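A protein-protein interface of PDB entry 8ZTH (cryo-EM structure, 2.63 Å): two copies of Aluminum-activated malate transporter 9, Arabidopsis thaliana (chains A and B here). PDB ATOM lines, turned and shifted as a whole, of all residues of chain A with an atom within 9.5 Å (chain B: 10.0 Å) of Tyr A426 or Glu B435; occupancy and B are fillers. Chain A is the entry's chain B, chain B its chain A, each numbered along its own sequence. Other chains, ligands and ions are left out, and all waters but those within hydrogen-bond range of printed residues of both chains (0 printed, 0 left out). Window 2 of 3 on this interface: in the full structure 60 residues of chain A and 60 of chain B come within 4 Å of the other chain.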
ATOM      1  N   ARG A 369     -24.378  -4.452 -30.026  1.00  0.00           N
ATOM      2  CA  ARG A 369     -25.241  -3.597 -29.220  1.00  0.00           C
ATOM      3  C   ARG A 369     -26.164  -4.421 -28.329  1.00  0.00           C
ATOM      4  O   ARG A 369     -26.415  -4.048 -27.178  1.00  0.00           O
ATOM      5  CB  ARG A 369     -26.048  -2.663 -30.119  1.00  0.00           C
ATOM      6  CG  ARG A 369     -25.200  -1.820 -31.056  1.00  0.00           C
ATOM      7  CD  ARG A 369     -25.785  -0.427 -31.220  1.00  0.00           C
ATOM      8  NE  ARG A 369     -24.749   0.587 -31.372  1.00  0.00           N
ATOM      9  CZ  ARG A 369     -24.735   1.506 -32.327  1.00  0.00           C
ATOM     10  NH1 ARG A 369     -25.692   1.571 -33.238  1.00  0.00           N
ATOM     11  NH2 ARG A 369     -23.737   2.384 -32.369  1.00  0.00           N
ATOM     12  N   VAL A 372     -24.968  -5.755 -24.759  1.00  0.00           N
ATOM     13  CA  VAL A 372     -24.796  -4.862 -23.619  1.00  0.00           C
ATOM     14  C   VAL A 372     -25.911  -4.996 -22.584  1.00  0.00           C
ATOM     15  O   VAL A 372     -25.743  -4.537 -21.445  1.00  0.00           O
ATOM     16  CB  VAL A 372     -24.697  -3.401 -24.100  1.00  0.00           C
ATOM     17  CG1 VAL A 372     -24.691  -2.441 -22.922  1.00  0.00           C
ATOM     18  CG2 VAL A 372     -23.455  -3.208 -24.952  1.00  0.00           C
ATOM     19  N   PHE A 373     -27.037  -5.623 -22.938  1.00  0.00           N
ATOM     20  CA  PHE A 373     -28.189  -5.740 -22.048  1.00  0.00           C
ATOM     21  C   PHE A 373     -28.522  -7.189 -21.701  1.00  0.00           C
ATOM     22  O   PHE A 373     -29.630  -7.469 -21.236  1.00  0.00           O
ATOM     23  CB  PHE A 373     -29.411  -5.061 -22.673  1.00  0.00           C
ATOM     24  CG  PHE A 373     -29.171  -3.639 -23.092  1.00  0.00           C
ATOM     25  CD1 PHE A 373     -28.692  -3.347 -24.358  1.00  0.00           C
ATOM     26  CD2 PHE A 373     -29.437  -2.592 -22.226  1.00  0.00           C
ATOM     27  CE1 PHE A 373     -28.474  -2.040 -24.750  1.00  0.00           C
ATOM     28  CE2 PHE A 373     -29.221  -1.282 -22.612  1.00  0.00           C
ATOM     29  CZ  PHE A 373     -28.740  -1.007 -23.876  1.00  0.00           C
ATOM     30  N   HIS A 419     -33.547   0.852 -15.304  1.00  0.00           N
ATOM     31  CA  HIS A 419     -32.400   1.667 -14.914  1.00  0.00           C
ATOM     32  C   HIS A 419     -31.244   1.505 -15.896  1.00  0.00           C
ATOM     33  O   HIS A 419     -30.620   2.493 -16.308  1.00  0.00           O
ATOM     34  CB  HIS A 419     -31.952   1.306 -13.499  1.00  0.00           C
ATOM     35  CG  HIS A 419     -32.713   2.017 -12.423  1.00  0.00           C
ATOM     36  ND1 HIS A 419     -33.286   1.358 -11.358  1.00  0.00           N
ATOM     37  CD2 HIS A 419     -32.990   3.330 -12.247  1.00  0.00           C
ATOM     38  CE1 HIS A 419     -33.886   2.234 -10.572  1.00  0.00           C
ATOM     39  NE2 HIS A 419     -33.722   3.439 -11.089  1.00  0.00           N
ATOM     40  N   LYS A 420     -30.949   0.264 -16.292  1.00  0.00           N
ATOM     41  CA  LYS A 420     -29.860   0.043 -17.236  1.00  0.00           C
ATOM     42  C   LYS A 420     -30.147   0.708 -18.576  1.00  0.00           C
ATOM     43  O   LYS A 420     -29.259   1.332 -19.170  1.00  0.00           O
ATOM     44  CB  LYS A 420     -29.609  -1.452 -17.421  1.00  0.00           C
ATOM     45  CG  LYS A 420     -28.458  -1.760 -18.364  1.00  0.00           C
ATOM     46  CD  LYS A 420     -27.120  -1.425 -17.728  1.00  0.00           C
ATOM     47  CE  LYS A 420     -25.964  -1.848 -18.618  1.00  0.00           C
ATOM     48  NZ  LYS A 420     -24.912  -2.576 -17.860  1.00  0.00           N
ATOM     49  N   ILE A 421     -31.382   0.588 -19.072  1.00  0.00           N
ATOM     50  CA  ILE A 421     -31.730   1.241 -20.331  1.00  0.00           C
ATOM     51  C   ILE A 421     -31.567   2.749 -20.211  1.00  0.00           C
ATOM     52  O   ILE A 421     -31.128   3.418 -21.154  1.00  0.00           O
ATOM     53  CB  ILE A 421     -33.159   0.859 -20.762  1.00  0.00           C
ATOM     54  CG1 ILE A 421     -33.125  -0.304 -21.753  1.00  0.00           C
ATOM     55  CG2 ILE A 421     -33.863   2.051 -21.383  1.00  0.00           C
ATOM     56  CD1 ILE A 421     -32.472  -1.549 -21.209  1.00  0.00           C
ATOM     57  N   ASP A 422     -31.918   3.311 -19.052  1.00  0.00           N
ATOM     58  CA  ASP A 422     -31.746   4.746 -18.854  1.00  0.00           C
ATOM     59  C   ASP A 422     -30.276   5.143 -18.824  1.00  0.00           C
ATOM     60  O   ASP A 422     -29.935   6.266 -19.211  1.00  0.00           O
ATOM     61  CB  ASP A 422     -32.432   5.189 -17.562  1.00  0.00           C
ATOM     62  CG  ASP A 422     -33.916   5.432 -17.744  1.00  0.00           C
ATOM     63  OD1 ASP A 422     -34.486   4.930 -18.735  1.00  0.00           O
ATOM     64  OD2 ASP A 422     -34.511   6.127 -16.895  1.00  0.00           O
ATOM     65  N   LYS A 423     -29.394   4.251 -18.370  1.00  0.00           N
ATOM     66  CA  LYS A 423     -27.984   4.610 -18.262  1.00  0.00           C
ATOM     67  C   LYS A 423     -27.230   4.554 -19.587  1.00  0.00           C
ATOM     68  O   LYS A 423     -26.199   5.223 -19.720  1.00  0.00           O
ATOM     69  CB  LYS A 423     -27.284   3.702 -17.248  1.00  0.00           C
ATOM     70  CG  LYS A 423     -26.888   4.399 -15.958  1.00  0.00           C
ATOM     71  CD  LYS A 423     -27.960   5.374 -15.500  1.00  0.00           C
ATOM     72  CE  LYS A 423     -29.117   4.651 -14.829  1.00  0.00           C
ATOM     73  NZ  LYS A 423     -30.126   5.598 -14.282  1.00  0.00           N
ATOM     74  N   LYS A 424     -27.706   3.787 -20.566  1.00  0.00           N
ATOM     75  CA  LYS A 424     -27.004   3.600 -21.833  1.00  0.00           C
ATOM     76  C   LYS A 424     -27.883   3.960 -23.025  1.00  0.00           C
ATOM     77  O   LYS A 424     -27.809   3.336 -24.085  1.00  0.00           O
ATOM     78  CB  LYS A 424     -26.495   2.167 -21.965  1.00  0.00           C
ATOM     79  CG  LYS A 424     -25.509   1.752 -20.889  1.00  0.00           C
ATOM     80  CD  LYS A 424     -24.087   1.777 -21.422  1.00  0.00           C
ATOM     81  CE  LYS A 424     -23.092   2.129 -20.331  1.00  0.00           C
ATOM     82  NZ  LYS A 424     -21.872   1.280 -20.401  1.00  0.00           N
ATOM     83  N   SER A 425     -28.725   4.981 -22.871  1.00  0.00           N
ATOM     84  CA  SER A 425     -29.680   5.333 -23.915  1.00  0.00           C
ATOM     85  C   SER A 425     -29.036   5.963 -25.145  1.00  0.00           C
ATOM     86  O   SER A 425     -29.723   6.132 -26.157  1.00  0.00           O
ATOM     87  CB  SER A 425     -30.738   6.282 -23.352  1.00  0.00           C
ATOM     88  OG  SER A 425     -31.734   6.549 -24.320  1.00  0.00           O
ATOM     89  N   TYR A 426     -27.748   6.313 -25.094  1.00  0.00           N
ATOM     90  CA  TYR A 426     -27.114   6.959 -26.237  1.00  0.00           C
ATOM     91  C   TYR A 426     -26.866   6.005 -27.401  1.00  0.00           C
ATOM     92  O   TYR A 426     -26.478   6.465 -28.480  1.00  0.00           O
ATOM     93  CB  TYR A 426     -25.801   7.626 -25.809  1.00  0.00           C
ATOM     94  CG  TYR A 426     -24.738   6.681 -25.293  1.00  0.00           C
ATOM     95  CD1 TYR A 426     -24.033   5.853 -26.158  1.00  0.00           C
ATOM     96  CD2 TYR A 426     -24.437   6.618 -23.940  1.00  0.00           C
ATOM     97  CE1 TYR A 426     -23.063   4.991 -25.690  1.00  0.00           C
ATOM     98  CE2 TYR A 426     -23.470   5.758 -23.463  1.00  0.00           C
ATOM     99  CZ  TYR A 426     -22.786   4.946 -24.342  1.00  0.00           C
ATOM    100  OH  TYR A 426     -21.820   4.089 -23.871  1.00  0.00           O
ATOM    101  N   LEU A 427     -27.077   4.705 -27.214  1.00  0.00           N
ATOM    102  CA  LEU A 427     -26.888   3.722 -28.269  1.00  0.00           C
ATOM    103  C   LEU A 427     -28.174   3.414 -29.026  1.00  0.00           C
ATOM    104  O   LEU A 427     -28.182   2.513 -29.871  1.00  0.00           O
ATOM    105  CB  LEU A 427     -26.311   2.428 -27.689  1.00  0.00           C
ATOM    106  CG  LEU A 427     -24.931   2.511 -27.037  1.00  0.00           C
ATOM    107  CD1 LEU A 427     -24.649   1.258 -26.226  1.00  0.00           C
ATOM    108  CD2 LEU A 427     -23.855   2.722 -28.090  1.00  0.00           C
ATOM    109  N   LEU A 428     -29.255   4.141 -28.748  1.00  0.00           N
ATOM    110  CA  LEU A 428     -30.538   3.915 -29.401  1.00  0.00           C
ATOM    111  C   LEU A 428     -30.963   5.046 -30.322  1.00  0.00           C
ATOM    112  O   LEU A 428     -31.627   4.786 -31.326  1.00  0.00           O
ATOM    113  CB  LEU A 428     -31.636   3.691 -28.353  1.00  0.00           C
ATOM    114  CG  LEU A 428     -31.357   2.611 -27.304  1.00  0.00           C
ATOM    115  CD1 LEU A 428     -32.405   2.652 -26.206  1.00  0.00           C
ATOM    116  CD2 LEU A 428     -31.299   1.234 -27.945  1.00  0.00           C
ATOM    117  N   VAL A 429     -30.595   6.273 -29.987  1.00  0.00           N
ATOM    118  CA  VAL A 429     -30.995   7.419 -30.778  1.00  0.00           C
ATOM    119  C   VAL A 429     -29.788   8.111 -31.369  1.00  0.00           C
ATOM    120  O   VAL A 429     -28.672   7.919 -30.898  1.00  0.00           O
ATOM    121  CB  VAL A 429     -31.770   8.424 -29.921  1.00  0.00           C
ATOM    122  CG1 VAL A 429     -33.085   7.823 -29.455  1.00  0.00           C
ATOM    123  CG2 VAL A 429     -30.926   8.868 -28.735  1.00  0.00           C
ATOM    124  N   ASN A 430     -30.001   8.910 -32.411  1.00  0.00           N
ATOM    125  CA  ASN A 430     -28.910   9.653 -33.034  1.00  0.00           C
ATOM    126  C   ASN A 430     -28.814  11.032 -32.414  1.00  0.00           C
ATOM    127  O   ASN A 430     -29.674  11.875 -32.649  1.00  0.00           O
ATOM    128  CB  ASN A 430     -29.143   9.773 -34.534  1.00  0.00           C
ATOM    129  CG  ASN A 430     -29.248   8.424 -35.216  1.00  0.00           C
ATOM    130  OD1 ASN A 430     -29.825   7.484 -34.673  1.00  0.00           O
ATOM    131  ND2 ASN A 430     -28.690   8.325 -36.416  1.00  0.00           N
ATOM    132  N   SER A 431     -27.777  11.275 -31.626  1.00  0.00           N
ATOM    133  CA  SER A 431     -27.671  12.549 -30.923  1.00  0.00           C
ATOM    134  C   SER A 431     -27.052  13.647 -31.769  1.00  0.00           C
ATOM    135  O   SER A 431     -27.181  14.827 -31.445  1.00  0.00           O
ATOM    136  CB  SER A 431     -26.856  12.369 -29.642  1.00  0.00           C
ATOM    137  OG  SER A 431     -26.538  13.622 -29.064  1.00  0.00           O
ATOM    138  N   GLU A 432     -26.389  13.272 -32.853  1.00  0.00           N
ATOM    139  CA  GLU A 432     -25.727  14.259 -33.697  1.00  0.00           C
ATOM    140  C   GLU A 432     -26.700  15.302 -34.224  1.00  0.00           C
ATOM    141  O   GLU A 432     -26.395  16.491 -34.225  1.00  0.00           O
ATOM    142  CB  GLU A 432     -25.028  13.568 -34.867  1.00  0.00           C
ATOM    143  CG  GLU A 432     -23.854  12.694 -34.454  1.00  0.00           C
ATOM    144  CD  GLU A 432     -23.228  11.965 -35.627  1.00  0.00           C
ATOM    145  OE1 GLU A 432     -23.817  11.987 -36.728  1.00  0.00           O
ATOM    146  OE2 GLU A 432     -22.144  11.370 -35.449  1.00  0.00           O
ATOM    147  N   TRP A 434     -30.103  17.269 -33.774  1.00  0.00           N
ATOM    148  CA  TRP A 434     -31.149  17.571 -32.807  1.00  0.00           C
ATOM    149  C   TRP A 434     -31.695  18.987 -32.893  1.00  0.00           C
ATOM    150  O   TRP A 434     -30.979  19.954 -32.638  1.00  0.00           O
ATOM    151  CB  TRP A 434     -30.657  17.288 -31.382  1.00  0.00           C
ATOM    152  CG  TRP A 434     -31.148  15.985 -30.860  1.00  0.00           C
ATOM    153  CD1 TRP A 434     -32.192  15.259 -31.343  1.00  0.00           C
ATOM    154  CD2 TRP A 434     -30.618  15.243 -29.758  1.00  0.00           C
ATOM    155  NE1 TRP A 434     -32.347  14.113 -30.613  1.00  0.00           N
ATOM    156  CE2 TRP A 434     -31.392  14.076 -29.634  1.00  0.00           C
ATOM    157  CE3 TRP A 434     -29.565  15.452 -28.865  1.00  0.00           C
ATOM    158  CZ2 TRP A 434     -31.149  13.119 -28.652  1.00  0.00           C
ATOM    159  CZ3 TRP A 434     -29.325  14.502 -27.890  1.00  0.00           C
ATOM    160  CH2 TRP A 434     -30.114  13.351 -27.792  1.00  0.00           C
ATOM    161  N   ALA A 534     -31.107   0.638 -34.788  1.00  0.00           N
ATOM    162  CA  ALA A 534     -30.930   1.134 -33.429  1.00  0.00           C
ATOM    163  C   ALA A 534     -32.227   1.049 -32.628  1.00  0.00           C
ATOM    164  O   ALA A 534     -32.206   0.695 -31.444  1.00  0.00           O
ATOM    165  CB  ALA A 534     -30.408   2.568 -33.458  1.00  0.00           C
ATOM    166  N   SER B 425     -35.317  13.026 -31.624  1.00  0.00           N
ATOM    167  CA  SER B 425     -35.117  11.840 -30.797  1.00  0.00           C
ATOM    168  C   SER B 425     -34.926  12.173 -29.321  1.00  0.00           C
ATOM    169  O   SER B 425     -35.063  11.280 -28.478  1.00  0.00           O
ATOM    170  CB  SER B 425     -33.914  11.044 -31.305  1.00  0.00           C
ATOM    171  OG  SER B 425     -32.735  11.830 -31.276  1.00  0.00           O
ATOM    172  N   LEU B 428     -37.620  11.060 -26.707  1.00  0.00           N
ATOM    173  CA  LEU B 428     -37.906   9.659 -26.441  1.00  0.00           C
ATOM    174  C   LEU B 428     -36.994   9.038 -25.394  1.00  0.00           C
ATOM    175  O   LEU B 428     -37.311   7.958 -24.886  1.00  0.00           O
ATOM    176  CB  LEU B 428     -37.804   8.844 -27.737  1.00  0.00           C
ATOM    177  CG  LEU B 428     -38.587   9.368 -28.943  1.00  0.00           C
ATOM    178  CD1 LEU B 428     -38.077   8.728 -30.223  1.00  0.00           C
ATOM    179  CD2 LEU B 428     -40.075   9.125 -28.774  1.00  0.00           C
ATOM    180  N   VAL B 429     -35.877   9.681 -25.058  1.00  0.00           N
ATOM    181  CA  VAL B 429     -34.935   9.161 -24.079  1.00  0.00           C
ATOM    182  C   VAL B 429     -34.635  10.245 -23.054  1.00  0.00           C
ATOM    183  O   VAL B 429     -34.987  11.412 -23.224  1.00  0.00           O
ATOM    184  CB  VAL B 429     -33.631   8.659 -24.732  1.00  0.00           C
ATOM    185  CG1 VAL B 429     -33.942   7.723 -25.889  1.00  0.00           C
ATOM    186  CG2 VAL B 429     -32.788   9.834 -25.198  1.00  0.00           C
ATOM    187  N   ASN B 430     -33.974   9.837 -21.975  1.00  0.00           N
ATOM    188  CA  ASN B 430     -33.529  10.745 -20.925  1.00  0.00           C
ATOM    189  C   ASN B 430     -32.032  10.968 -21.093  1.00  0.00           C
ATOM    190  O   ASN B 430     -31.244  10.024 -20.960  1.00  0.00           O
ATOM    191  CB  ASN B 430     -33.840  10.181 -19.538  1.00  0.00           C
ATOM    192  CG  ASN B 430     -35.328  10.055 -19.279  1.00  0.00           C
ATOM    193  OD1 ASN B 430     -35.974   9.113 -19.739  1.00  0.00           O
ATOM    194  ND2 ASN B 430     -35.882  11.007 -18.536  1.00  0.00           N
ATOM    195  N   SER B 431     -31.626  12.194 -21.390  1.00  0.00           N
ATOM    196  CA  SER B 431     -30.216  12.453 -21.660  1.00  0.00           C
ATOM    197  C   SER B 431     -29.472  13.020 -20.466  1.00  0.00           C
ATOM    198  O   SER B 431     -28.362  13.527 -20.607  1.00  0.00           O
ATOM    199  CB  SER B 431     -30.091  13.416 -22.836  1.00  0.00           C
ATOM    200  OG  SER B 431     -30.650  14.678 -22.525  1.00  0.00           O
ATOM    201  N   GLU B 432     -30.073  12.940 -19.291  1.00  0.00           N
ATOM    202  CA  GLU B 432     -29.450  13.499 -18.104  1.00  0.00           C
ATOM    203  C   GLU B 432     -28.789  12.418 -17.282  1.00  0.00           C
ATOM    204  O   GLU B 432     -28.263  12.692 -16.208  1.00  0.00           O
ATOM    205  CB  GLU B 432     -30.497  14.216 -17.261  1.00  0.00           C
ATOM    206  CG  GLU B 432     -31.590  13.304 -16.728  1.00  0.00           C
ATOM    207  CD  GLU B 432     -32.683  14.059 -15.995  1.00  0.00           C
ATOM    208  OE1 GLU B 432     -32.450  15.221 -15.599  1.00  0.00           O
ATOM    209  OE2 GLU B 432     -33.779  13.490 -15.816  1.00  0.00           O
ATOM    210  N   CYS B 433     -28.817  11.188 -17.775  1.00  0.00           N
ATOM    211  CA  CYS B 433     -28.251  10.074 -17.029  1.00  0.00           C
ATOM    212  C   CYS B 433     -27.198   9.357 -17.832  1.00  0.00           C
ATOM    213  O   CYS B 433     -26.719   8.303 -17.424  1.00  0.00           O
ATOM    214  CB  CYS B 433     -29.357   9.086 -16.667  1.00  0.00           C
ATOM    215  SG  CYS B 433     -30.605   9.734 -15.535  1.00  0.00           S
ATOM    216  N   TRP B 434     -26.824   9.914 -18.971  1.00  0.00           N
ATOM    217  CA  TRP B 434     -25.897   9.212 -19.849  1.00  0.00           C
ATOM    218  C   TRP B 434     -24.529   8.996 -19.223  1.00  0.00           C
ATOM    219  O   TRP B 434     -23.912   9.934 -18.724  1.00  0.00           O
ATOM    220  CB  TRP B 434     -25.793   9.942 -21.188  1.00  0.00           C
ATOM    221  CG  TRP B 434     -26.975   9.667 -22.060  1.00  0.00           C
ATOM    222  CD1 TRP B 434     -27.973   8.770 -21.821  1.00  0.00           C
ATOM    223  CD2 TRP B 434     -27.288  10.291 -23.309  1.00  0.00           C
ATOM    224  NE1 TRP B 434     -28.888   8.796 -22.840  1.00  0.00           N
ATOM    225  CE2 TRP B 434     -28.491   9.721 -23.769  1.00  0.00           C
ATOM    226  CE3 TRP B 434     -26.669  11.276 -24.083  1.00  0.00           C
ATOM    227  CZ2 TRP B 434     -29.087  10.102 -24.966  1.00  0.00           C
ATOM    228  CZ3 TRP B 434     -27.262  11.652 -25.273  1.00  0.00           C
ATOM    229  CH2 TRP B 434     -28.458  11.067 -25.702  1.00  0.00           C
ATOM    230  N   GLU B 435     -24.062   7.753 -19.249  1.00  0.00           N
ATOM    231  CA  GLU B 435     -22.762   7.431 -18.680  1.00  0.00           C
ATOM    232  C   GLU B 435     -22.047   6.408 -19.547  1.00  0.00           C
ATOM    233  O   GLU B 435     -22.676   5.524 -20.126  1.00  0.00           O
ATOM    234  CB  GLU B 435     -22.923   6.887 -17.265  1.00  0.00           C
ATOM    235  CG  GLU B 435     -23.966   5.790 -17.142  1.00  0.00           C
ATOM    236  CD  GLU B 435     -23.402   4.409 -17.419  1.00  0.00           C
ATOM    237  OE1 GLU B 435     -22.165   4.246 -17.362  1.00  0.00           O
ATOM    238  OE2 GLU B 435     -24.196   3.484 -17.695  1.00  0.00           O
ATOM    239  N   LEU B 535     -40.633   5.721 -24.172  1.00  0.00           N
ATOM    240  CA  LEU B 535     -40.109   4.717 -25.091  1.00  0.00           C
ATOM    241  C   LEU B 535     -41.183   4.009 -25.916  1.00  0.00           C
ATOM    242  O   LEU B 535     -40.836   3.332 -26.888  1.00  0.00           O
ATOM    243  CB  LEU B 535     -39.302   3.675 -24.312  1.00  0.00           C
ATOM    244  CG  LEU B 535     -38.012   3.173 -24.962  1.00  0.00           C
ATOM    245  CD1 LEU B 535     -37.034   4.315 -25.171  1.00  0.00           C
ATOM    246  CD2 LEU B 535     -37.385   2.074 -24.121  1.00  0.00           C
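NE1 of Trp A434 lies within hydrogen-bond range of OG of Ser B425, 2.4 Å away. The backbone NH (N) of Glu B435 lies within hydrogen-bond range of the backbone carbonyl oxygen (O) of Lys A423, at 3.3 Å. The backbone carbonyl oxygen (O) of Asn A430 lies within hydrogen-bond range of the side-chain hydroxyl (OG) of Ser B425, at 3.4 Å.
NE1 of Trp B434 lies within hydrogen-bond range of O of Asn B430, at 3.3 Å.
Of chain B, only Glu B435 comes within 4 Å of Lys A424. Tyr A426 touches two residues of chain B. Printed residues of chain A within 4 Å of Cys B433: Asp A422 (3.8 Å) and Lys A423 (3.7 Å). Of the printed residues of chain A, Trp B434 touches Ser A425, Tyr A426 and Trp A434. Glu B435 touches just these residues of chain A: Lys A423, Lys A424 and Tyr A426. The nearest printed residue of chain B that does not touch Lys A423 is Trp B434 (4.002 Å).
Of the 10 printed residues of chain B, 5 touch a printed residue of chain A. Along chain B the printed residues that touch a printed residue of chain A span positions 425 to 435. Of the 19 printed residues of chain A, 8 touch a printed residue of chain B. Hydrophobic or aromatic side chains of chain A within 4 Å of the printed part of chain B: Tyr A426, Val A429 and Trp A434.
Among the printed residues, pairs that only touch across the chains: Ser A425 with Val B429, Lys A424 with Glu B435, Ser A425 with Trp B434, Tyr A426 with Glu B435, Trp A434 with Trp B434, Tyr A426 with Trp B434, Val A429 with Ser B425, Val A429 with Val B429, Lys A423 with Cys B433 and Asp A422 with Cys B433.
Ser A425 touches Val B429, and with the chains exchanged Val A429 touches Ser B425. Ser A425 touches Trp B434, and with the chains exchanged Trp A434 touches Ser B425. Val A429 touches its own counterpart, Val B429. Trp B434 touches its own counterpart, Trp A434. Positions printed for both chains: 425, 428, 429, 430, 431, 432 and 434. Of the 13 pairs that touch across the chains among the printed residues, 6 have their exchanged pair printed and touching as well.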
